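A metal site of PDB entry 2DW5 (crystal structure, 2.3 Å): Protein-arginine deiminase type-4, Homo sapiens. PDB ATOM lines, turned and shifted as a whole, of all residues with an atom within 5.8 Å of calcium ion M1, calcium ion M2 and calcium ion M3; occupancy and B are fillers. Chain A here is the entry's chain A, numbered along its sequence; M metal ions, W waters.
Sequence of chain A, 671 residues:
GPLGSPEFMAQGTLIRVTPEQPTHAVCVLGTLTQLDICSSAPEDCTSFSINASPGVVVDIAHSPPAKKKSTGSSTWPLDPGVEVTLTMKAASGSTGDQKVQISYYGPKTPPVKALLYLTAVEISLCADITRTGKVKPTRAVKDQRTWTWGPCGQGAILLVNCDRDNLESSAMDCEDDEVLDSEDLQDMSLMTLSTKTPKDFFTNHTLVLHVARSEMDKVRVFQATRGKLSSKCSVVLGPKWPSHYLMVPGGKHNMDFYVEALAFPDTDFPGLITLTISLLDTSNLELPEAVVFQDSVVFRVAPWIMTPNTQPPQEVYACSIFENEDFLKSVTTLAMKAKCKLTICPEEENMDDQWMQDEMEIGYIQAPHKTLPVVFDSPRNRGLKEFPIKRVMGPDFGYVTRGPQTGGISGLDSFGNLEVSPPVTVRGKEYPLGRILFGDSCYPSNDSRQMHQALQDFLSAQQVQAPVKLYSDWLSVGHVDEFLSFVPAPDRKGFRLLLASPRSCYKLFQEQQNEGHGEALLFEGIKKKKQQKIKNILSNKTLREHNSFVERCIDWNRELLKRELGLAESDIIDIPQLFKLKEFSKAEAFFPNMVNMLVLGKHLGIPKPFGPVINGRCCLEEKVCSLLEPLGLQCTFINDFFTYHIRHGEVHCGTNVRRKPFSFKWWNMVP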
ATOM      1  N   ASN A 161       0.672  12.550  -1.845  1.00  0.00           N
ATOM      2  CA  ASN A 161       1.545  12.524  -0.671  1.00  0.00           C
ATOM      3  C   ASN A 161       2.458  13.753  -0.584  1.00  0.00           C
ATOM      4  O   ASN A 161       3.678  13.678  -0.505  1.00  0.00           O
ATOM      5  CB  ASN A 161       2.281  11.186  -0.563  1.00  0.00           C
ATOM      6  CG  ASN A 161       2.897  10.926   0.836  1.00  0.00           C
ATOM      7  OD1 ASN A 161       2.748  11.732   1.771  1.00  0.00           O
ATOM      8  ND2 ASN A 161       3.604   9.815   0.957  1.00  0.00           N
ATOM      9  N   CYS A 162       1.804  14.902  -0.473  1.00  0.00           N
ATOM     10  CA  CYS A 162       2.401  16.200  -0.706  1.00  0.00           C
ATOM     11  C   CYS A 162       2.713  16.940   0.575  1.00  0.00           C
ATOM     12  O   CYS A 162       2.921  18.156   0.541  1.00  0.00           O
ATOM     13  CB  CYS A 162       1.420  17.049  -1.513  1.00  0.00           C
ATOM     14  SG  CYS A 162      -0.114  17.359  -0.641  1.00  0.00           S
ATOM     15  N   ASP A 163       2.703  16.215   1.698  1.00  0.00           N
ATOM     16  CA  ASP A 163       3.170  16.741   2.972  1.00  0.00           C
ATOM     17  C   ASP A 163       4.615  16.277   3.230  1.00  0.00           C
ATOM     18  O   ASP A 163       5.239  15.631   2.377  1.00  0.00           O
ATOM     19  CB  ASP A 163       2.205  16.370   4.113  1.00  0.00           C
ATOM     20  CG  ASP A 163       2.340  14.927   4.585  1.00  0.00           C
ATOM     21  OD1 ASP A 163       2.737  14.025   3.790  1.00  0.00           O
ATOM     22  OD2 ASP A 163       2.043  14.710   5.796  1.00  0.00           O
ATOM     23  N   ARG A 164       5.140  16.650   4.399  1.00  0.00           N
ATOM     24  CA  ARG A 164       6.562  16.413   4.732  1.00  0.00           C
ATOM     25  C   ARG A 164       6.704  15.912   6.168  1.00  0.00           C
ATOM     26  O   ARG A 164       6.942  16.685   7.093  1.00  0.00           O
ATOM     27  CB  ARG A 164       7.393  17.682   4.536  1.00  0.00           C
ATOM     28  CG  ARG A 164       8.891  17.482   4.610  1.00  0.00           C
ATOM     29  CD  ARG A 164       9.665  18.722   4.182  1.00  0.00           C
ATOM     30  NE  ARG A 164       9.900  19.598   5.326  1.00  0.00           N
ATOM     31  CZ  ARG A 164       9.489  20.868   5.442  1.00  0.00           C
ATOM     32  NH1 ARG A 164       8.823  21.498   4.477  1.00  0.00           N
ATOM     33  NH2 ARG A 164       9.769  21.520   6.559  1.00  0.00           N
ATOM     34  N   ASP A 165       6.530  14.597   6.339  1.00  0.00           N
ATOM     35  CA  ASP A 165       6.756  13.924   7.618  1.00  0.00           C
ATOM     36  C   ASP A 165       8.250  13.742   7.927  1.00  0.00           C
ATOM     37  O   ASP A 165       8.623  13.588   9.090  1.00  0.00           O
ATOM     38  CB  ASP A 165       6.052  12.539   7.648  1.00  0.00           C
ATOM     39  CG  ASP A 165       4.538  12.633   7.453  1.00  0.00           C
ATOM     40  OD1 ASP A 165       3.859  13.374   8.204  1.00  0.00           O
ATOM     41  OD2 ASP A 165       4.042  11.960   6.533  1.00  0.00           O
ATOM     42  N   ASP A 173       7.125  14.308   0.729  1.00  0.00           N
ATOM     43  CA  ASP A 173       7.509  12.892   0.883  1.00  0.00           C
ATOM     44  C   ASP A 173       7.438  12.086  -0.427  1.00  0.00           C
ATOM     45  O   ASP A 173       8.188  11.137  -0.582  1.00  0.00           O
ATOM     46  CB  ASP A 173       6.655  12.186   1.935  1.00  0.00           C
ATOM     47  CG  ASP A 173       6.672  12.873   3.309  1.00  0.00           C
ATOM     48  OD1 ASP A 173       7.749  13.304   3.800  1.00  0.00           O
ATOM     49  OD2 ASP A 173       5.595  12.970   3.904  1.00  0.00           O
ATOM     50  N   CYS A 174       6.524  12.451  -1.349  1.00  0.00           N
ATOM     51  CA  CYS A 174       6.346  11.690  -2.597  1.00  0.00           C
ATOM     52  C   CYS A 174       7.303  12.046  -3.744  1.00  0.00           C
ATOM     53  O   CYS A 174       7.143  11.574  -4.876  1.00  0.00           O
ATOM     54  CB  CYS A 174       4.911  11.803  -3.110  1.00  0.00           C
ATOM     55  SG  CYS A 174       4.475  13.466  -3.685  1.00  0.00           S
ATOM     56  N   GLU A 175       8.324  12.857  -3.461  1.00  0.00           N
ATOM     57  CA  GLU A 175       9.279  13.193  -4.511  1.00  0.00           C
ATOM     58  C   GLU A 175      10.408  12.145  -4.662  1.00  0.00           C
ATOM     59  O   GLU A 175      11.072  12.121  -5.705  1.00  0.00           O
ATOM     60  CB  GLU A 175       9.797  14.615  -4.319  1.00  0.00           C
ATOM     61  CG  GLU A 175       8.716  15.648  -4.659  1.00  0.00           C
ATOM     62  CD  GLU A 175       9.121  17.102  -4.401  1.00  0.00           C
ATOM     63  OE1 GLU A 175      10.018  17.333  -3.540  1.00  0.00           O
ATOM     64  OE2 GLU A 175       8.538  18.006  -5.052  1.00  0.00           O
ATOM     65  N   ASP A 176      10.597  11.283  -3.661  1.00  0.00           N
ATOM     66  CA  ASP A 176      11.566  10.175  -3.752  1.00  0.00           C
ATOM     67  C   ASP A 176      10.796   8.875  -3.882  1.00  0.00           C
ATOM     68  O   ASP A 176       9.534   8.882  -3.867  1.00  0.00           O
ATOM     69  CB  ASP A 176      12.487  10.142  -2.523  1.00  0.00           C
ATOM     70  CG  ASP A 176      11.756   9.801  -1.222  1.00  0.00           C
ATOM     71  OD1 ASP A 176      12.286  10.101  -0.133  1.00  0.00           O
ATOM     72  OD2 ASP A 176      10.642   9.224  -1.255  1.00  0.00           O
ATOM     73  N   ASP A 177      11.526   7.764  -3.982  1.00  0.00           N
ATOM     74  CA  ASP A 177      10.896   6.428  -4.119  1.00  0.00           C
ATOM     75  C   ASP A 177      11.143   5.551  -2.897  1.00  0.00           C
ATOM     76  O   ASP A 177      11.543   4.384  -3.011  1.00  0.00           O
ATOM     77  CB  ASP A 177      11.312   5.723  -5.420  1.00  0.00           C
ATOM     78  CG  ASP A 177      12.664   6.165  -5.930  1.00  0.00           C
ATOM     79  OD1 ASP A 177      13.718   5.618  -5.483  1.00  0.00           O
ATOM     80  OD2 ASP A 177      12.676   7.062  -6.809  1.00  0.00           O
ATOM     81  N   GLU A 178      10.866   6.108  -1.715  1.00  0.00           N
ATOM     82  CA  GLU A 178      11.101   5.437  -0.439  1.00  0.00           C
ATOM     83  C   GLU A 178      10.118   5.866   0.644  1.00  0.00           C
ATOM     84  O   GLU A 178       9.779   7.044   0.755  1.00  0.00           O
ATOM     85  CB  GLU A 178      12.491   5.797   0.043  1.00  0.00           C
ATOM     86  CG  GLU A 178      13.585   5.254  -0.821  1.00  0.00           C
ATOM     87  CD  GLU A 178      14.926   5.406  -0.156  1.00  0.00           C
ATOM     88  OE1 GLU A 178      15.086   4.893   0.979  1.00  0.00           O
ATOM     89  OE2 GLU A 178      15.813   6.030  -0.775  1.00  0.00           O
ATOM     90  N   VAL A 179       9.703   4.915   1.480  1.00  0.00           N
ATOM     91  CA  VAL A 179       8.953   5.251   2.684  1.00  0.00           C
ATOM     92  C   VAL A 179      10.002   5.513   3.772  1.00  0.00           C
ATOM     93  O   VAL A 179      10.583   4.559   4.298  1.00  0.00           O
ATOM     94  CB  VAL A 179       7.963   4.136   3.106  1.00  0.00           C
ATOM     95  CG1 VAL A 179       7.079   4.609   4.255  1.00  0.00           C
ATOM     96  CG2 VAL A 179       7.085   3.734   1.953  1.00  0.00           C
ATOM     97  N   LEU A 180      10.254   6.779   4.082  1.00  0.00           N
ATOM     98  CA  LEU A 180      11.376   7.151   4.991  1.00  0.00           C
ATOM     99  C   LEU A 180      10.996   7.108   6.451  1.00  0.00           C
ATOM    100  O   LEU A 180      11.842   6.903   7.313  1.00  0.00           O
ATOM    101  CB  LEU A 180      11.933   8.542   4.675  1.00  0.00           C
ATOM    102  CG  LEU A 180      12.869   8.626   3.471  1.00  0.00           C
ATOM    103  CD1 LEU A 180      13.375  10.076   3.339  1.00  0.00           C
ATOM    104  CD2 LEU A 180      14.023   7.595   3.539  1.00  0.00           C
ATOM    105  N   GLU A 183       5.359   6.825   9.929  1.00  0.00           N
ATOM    106  CA  GLU A 183       4.212   7.738   9.914  1.00  0.00           C
ATOM    107  C   GLU A 183       3.727   8.087   8.505  1.00  0.00           C
ATOM    108  O   GLU A 183       2.555   8.357   8.309  1.00  0.00           O
ATOM    109  CB  GLU A 183       4.541   9.062  10.623  1.00  0.00           C
ATOM    110  CG  GLU A 183       4.754   8.947  12.117  1.00  0.00           C
ATOM    111  CD  GLU A 183       6.180   8.587  12.483  1.00  0.00           C
ATOM    112  OE1 GLU A 183       6.485   8.640  13.690  1.00  0.00           O
ATOM    113  OE2 GLU A 183       6.983   8.245  11.580  1.00  0.00           O
ATOM    114  N   ASP A 184       4.658   8.106   7.552  1.00  0.00           N
ATOM    115  CA  ASP A 184       4.374   8.412   6.158  1.00  0.00           C
ATOM    116  C   ASP A 184       3.321   7.455   5.588  1.00  0.00           C
ATOM    117  O   ASP A 184       2.484   7.881   4.754  1.00  0.00           O
ATOM    118  CB  ASP A 184       5.653   8.364   5.301  1.00  0.00           C
ATOM    119  CG  ASP A 184       5.422   8.775   3.825  1.00  0.00           C
ATOM    120  OD1 ASP A 184       5.977   8.128   2.911  1.00  0.00           O
ATOM    121  OD2 ASP A 184       4.694   9.754   3.568  1.00  0.00           O
ATOM    122  N   GLN A 186       0.724   6.339   6.913  1.00  0.00           N
ATOM    123  CA  GLN A 186      -0.611   6.763   7.283  1.00  0.00           C
ATOM    124  C   GLN A 186      -1.245   7.604   6.199  1.00  0.00           C
ATOM    125  O   GLN A 186      -2.475   7.650   6.087  1.00  0.00           O
ATOM    126  CB  GLN A 186      -0.569   7.540   8.614  1.00  0.00           C
ATOM    127  CG  GLN A 186      -0.105   6.706   9.810  1.00  0.00           C
ATOM    128  CD  GLN A 186       0.197   7.555  11.061  1.00  0.00           C
ATOM    129  OE1 GLN A 186       0.927   7.111  11.968  1.00  0.00           O
ATOM    130  NE2 GLN A 186      -0.355   8.775  11.108  1.00  0.00           N
ATOM    131  N   ASP A 187      -0.440   8.282   5.399  1.00  0.00           N
ATOM    132  CA  ASP A 187      -0.994   9.052   4.283  1.00  0.00           C
ATOM    133  C   ASP A 187      -1.327   8.158   3.109  1.00  0.00           C
ATOM    134  O   ASP A 187      -2.089   8.564   2.245  1.00  0.00           O
ATOM    135  CB  ASP A 187      -0.054  10.153   3.811  1.00  0.00           C
ATOM    136  CG  ASP A 187       0.297  11.108   4.919  1.00  0.00           C
ATOM    137  OD1 ASP A 187      -0.542  11.414   5.804  1.00  0.00           O
ATOM    138  OD2 ASP A 187       1.452  11.536   4.922  1.00  0.00           O
ATOM    139  N   MET A 188      -0.787   6.939   3.104  1.00  0.00           N
ATOM    140  CA  MET A 188      -0.916   6.037   1.958  1.00  0.00           C
ATOM    141  C   MET A 188      -2.112   5.116   2.057  1.00  0.00           C
ATOM    142  O   MET A 188      -2.623   4.888   3.122  1.00  0.00           O
ATOM    143  CB  MET A 188       0.362   5.224   1.807  1.00  0.00           C
ATOM    144  CG  MET A 188       1.550   6.092   1.647  1.00  0.00           C
ATOM    145  SD  MET A 188       2.963   5.175   1.058  1.00  0.00           S
ATOM    146  CE  MET A 188       4.226   6.357   1.464  1.00  0.00           C
ATOM    147  N   ARG A 220       2.726   5.853  -6.918  1.00  0.00           N
ATOM    148  CA  ARG A 220       3.843   5.005  -6.486  1.00  0.00           C
ATOM    149  C   ARG A 220       3.304   3.948  -5.546  1.00  0.00           C
ATOM    150  O   ARG A 220       2.375   4.217  -4.773  1.00  0.00           O
ATOM    151  CB  ARG A 220       4.936   5.825  -5.845  1.00  0.00           C
ATOM    152  CG  ARG A 220       6.161   4.970  -5.514  1.00  0.00           C
ATOM    153  CD  ARG A 220       7.259   5.768  -4.973  1.00  0.00           C
ATOM    154  NE  ARG A 220       7.834   6.624  -5.994  1.00  0.00           N
ATOM    155  CZ  ARG A 220       7.698   7.935  -6.068  1.00  0.00           C
ATOM    156  NH1 ARG A 220       6.992   8.614  -5.155  1.00  0.00           N
ATOM    157  NH2 ARG A 220       8.299   8.602  -7.058  1.00  0.00           N
ATOM    158  N   PHE A 222       4.362   0.720  -2.907  1.00  0.00           N
ATOM    159  CA  PHE A 222       5.382   0.034  -2.117  1.00  0.00           C
ATOM    160  C   PHE A 222       4.855  -1.324  -1.627  1.00  0.00           C
ATOM    161  O   PHE A 222       3.678  -1.474  -1.339  1.00  0.00           O
ATOM    162  CB  PHE A 222       5.769   0.868  -0.889  1.00  0.00           C
ATOM    163  CG  PHE A 222       6.366   2.229  -1.216  1.00  0.00           C
ATOM    164  CD1 PHE A 222       5.548   3.361  -1.363  1.00  0.00           C
ATOM    165  CD2 PHE A 222       7.743   2.375  -1.353  1.00  0.00           C
ATOM    166  CE1 PHE A 222       6.109   4.628  -1.655  1.00  0.00           C
ATOM    167  CE2 PHE A 222       8.292   3.637  -1.652  1.00  0.00           C
ATOM    168  CZ  PHE A 222       7.481   4.750  -1.797  1.00  0.00           C
ATOM    169  N   GLU A 260       0.530   5.744  -2.902  1.00  0.00           N
ATOM    170  CA  GLU A 260       0.479   7.204  -2.731  1.00  0.00           C
ATOM    171  C   GLU A 260       0.286   7.783  -4.091  1.00  0.00           C
ATOM    172  O   GLU A 260       0.818   7.239  -5.051  1.00  0.00           O
ATOM    173  CB  GLU A 260       1.799   7.724  -2.145  1.00  0.00           C
ATOM    174  CG  GLU A 260       3.090   7.307  -2.912  1.00  0.00           C
ATOM    175  CD  GLU A 260       4.333   7.977  -2.351  1.00  0.00           C
ATOM    176  OE1 GLU A 260       4.267   8.507  -1.222  1.00  0.00           O
ATOM    177  OE2 GLU A 260       5.390   7.995  -3.006  1.00  0.00           O
ATOM    178  N   LYS A 370      -7.516   9.202   6.376  1.00  0.00           N
ATOM    179  CA  LYS A 370      -6.601  10.345   6.624  1.00  0.00           C
ATOM    180  C   LYS A 370      -7.120  11.649   5.978  1.00  0.00           C
ATOM    181  O   LYS A 370      -7.461  11.694   4.799  1.00  0.00           O
ATOM    182  CB  LYS A 370      -5.178  10.029   6.093  1.00  0.00           C
ATOM    183  CG  LYS A 370      -4.059  10.987   6.579  1.00  0.00           C
ATOM    184  CD  LYS A 370      -3.835  10.859   8.104  1.00  0.00           C
ATOM    185  CE  LYS A 370      -2.412  11.238   8.566  1.00  0.00           C
ATOM    186  NZ  LYS A 370      -1.930  10.397   9.739  1.00  0.00           N
ATOM    187  N   LEU A 372      -5.810  15.737   5.794  1.00  0.00           N
ATOM    188  CA  LEU A 372      -4.794  16.705   6.223  1.00  0.00           C
ATOM    189  C   LEU A 372      -4.917  18.054   5.581  1.00  0.00           C
ATOM    190  O   LEU A 372      -5.430  18.156   4.484  1.00  0.00           O
ATOM    191  CB  LEU A 372      -3.389  16.187   6.014  1.00  0.00           C
ATOM    192  CG  LEU A 372      -2.908  15.683   4.672  1.00  0.00           C
ATOM    193  CD1 LEU A 372      -1.504  16.246   4.367  1.00  0.00           C
ATOM    194  CD2 LEU A 372      -2.852  14.193   4.754  1.00  0.00           C
ATOM    195  N   PRO A 395       4.942  18.256   8.744  1.00  0.00           N
ATOM    196  CA  PRO A 395       4.251  17.089   9.257  1.00  0.00           C
ATOM    197  C   PRO A 395       2.744  17.257   9.284  1.00  0.00           C
ATOM    198  O   PRO A 395       2.224  18.059  10.058  1.00  0.00           O
ATOM    199  CB  PRO A 395       4.816  16.944  10.695  1.00  0.00           C
ATOM    200  CG  PRO A 395       6.183  17.541  10.596  1.00  0.00           C
ATOM    201  CD  PRO A 395       5.951  18.744   9.702  1.00  0.00           C
ATOM    202  N   ASP A 396       2.087  16.491   8.421  1.00  0.00           N
ATOM    203  CA  ASP A 396       0.626  16.523   8.269  1.00  0.00           C
ATOM    204  C   ASP A 396       0.122  17.876   7.797  1.00  0.00           C
ATOM    205  O   ASP A 396      -0.980  18.314   8.124  1.00  0.00           O
ATOM    206  CB  ASP A 396      -0.097  15.985   9.514  1.00  0.00           C
ATOM    207  CG  ASP A 396       0.012  14.454   9.625  1.00  0.00           C
ATOM    208  OD1 ASP A 396       0.041  13.792   8.569  1.00  0.00           O
ATOM    209  OD2 ASP A 396       0.086  13.898  10.743  1.00  0.00           O
HETATM  210 CA    CA M   1       3.560  11.863   4.073  1.00  0.00          CA
HETATM  211 CA    CA M   2       1.433  12.543   7.211  1.00  0.00          CA
HETATM  212 CA    CA M   3       8.734   8.972   0.030  1.00  0.00          CA
HETATM  213  O   HOH W   1       7.878   8.212  -1.967  1.00  0.00           O
HETATM  214  O   HOH W   2       6.072   8.890   0.432  1.00  0.00           O
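The guanidinium group (NH1) of Arg 220 is in hydrogen-bond range of the backbone carbonyl oxygen (O) of Asp 176 (2.9 Å).
The side-chain amide nitrogen (ND2) of Asn 161 sits at hydrogen-bond distance from the side-chain carboxylate (OE1) of Glu 260 (2.6 Å).
O of Asn 161 is in hydrogen-bond range of N of Cys 174 (3.2 Å).
Six residues have an atom within 4 Å of calcium ion M1: Asn 161, Asp 163, Asp 165, Asp 173, Asp 184 and Asp 187.
The nearest printed residue that does not touch calcium ion M1 is Arg 164 (5.1 Å).
Along chain A the residues within 4 Å of calcium ion M2 span positions 163 to 396.
Within 4 Å of calcium ion M3: Asp 173, Asp 176 and Glu 178.
The nearest printed residue that does not touch calcium ion M3 is Asp 184 (4.1 Å).
The side-chain carboxylate (OD2) of Asp 187 is bound to calcium ion M1, at 2.3 Å.
The side-chain carboxylate (OD2) of Asp 173 is bound to calcium ion M1.
Calcium ion M1 is bound by OD1 of Asp 163 (2.3 Å).
Calcium ion M1 is bound by OD1 of Asn 161.
Calcium ion M1 is bound by the side-chain carboxylate (OD2) of Asp 184, 2.4 Å away.
The side-chain carboxylate (OD2) of Asp 165 binds calcium ion M1, at 2.5 Å.
Calcium ion M1 has six donor atoms within binding distance.
Calcium ion M2 is bound by OD1 of Asp 396 (2.3 Å), OD2 of Asp 187 (2.5 Å), OD2 of Asp 163 (2.7 Å), OD1 of Asp 187 (2.7 Å), OD1 of Asp 165 (2.7 Å) and OD2 of Asp 165 (2.8 Å).
Water W1 binds calcium ion M3.
The backbone carbonyl oxygen (O) of Glu 178 is bound to calcium ion M3 (2.3 Å).
The side-chain carboxylate (OD2) of Asp 176 is bound to calcium ion M3 (2.3 Å).
Calcium ion M3 is bound by O of Asp 173.
Calcium ion M3 is bound by water W2.
Water W1 lies within hydrogen-bond range of O of Asp 176 (2.6 Å), OE2 of Glu 260 (2.7 Å) and NH1 of Arg 220 (3.3 Å).
Water W2 lies within hydrogen-bond range of OE1 of Glu 260, OD1 of Asp 184 and ND2 of Asn 161.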
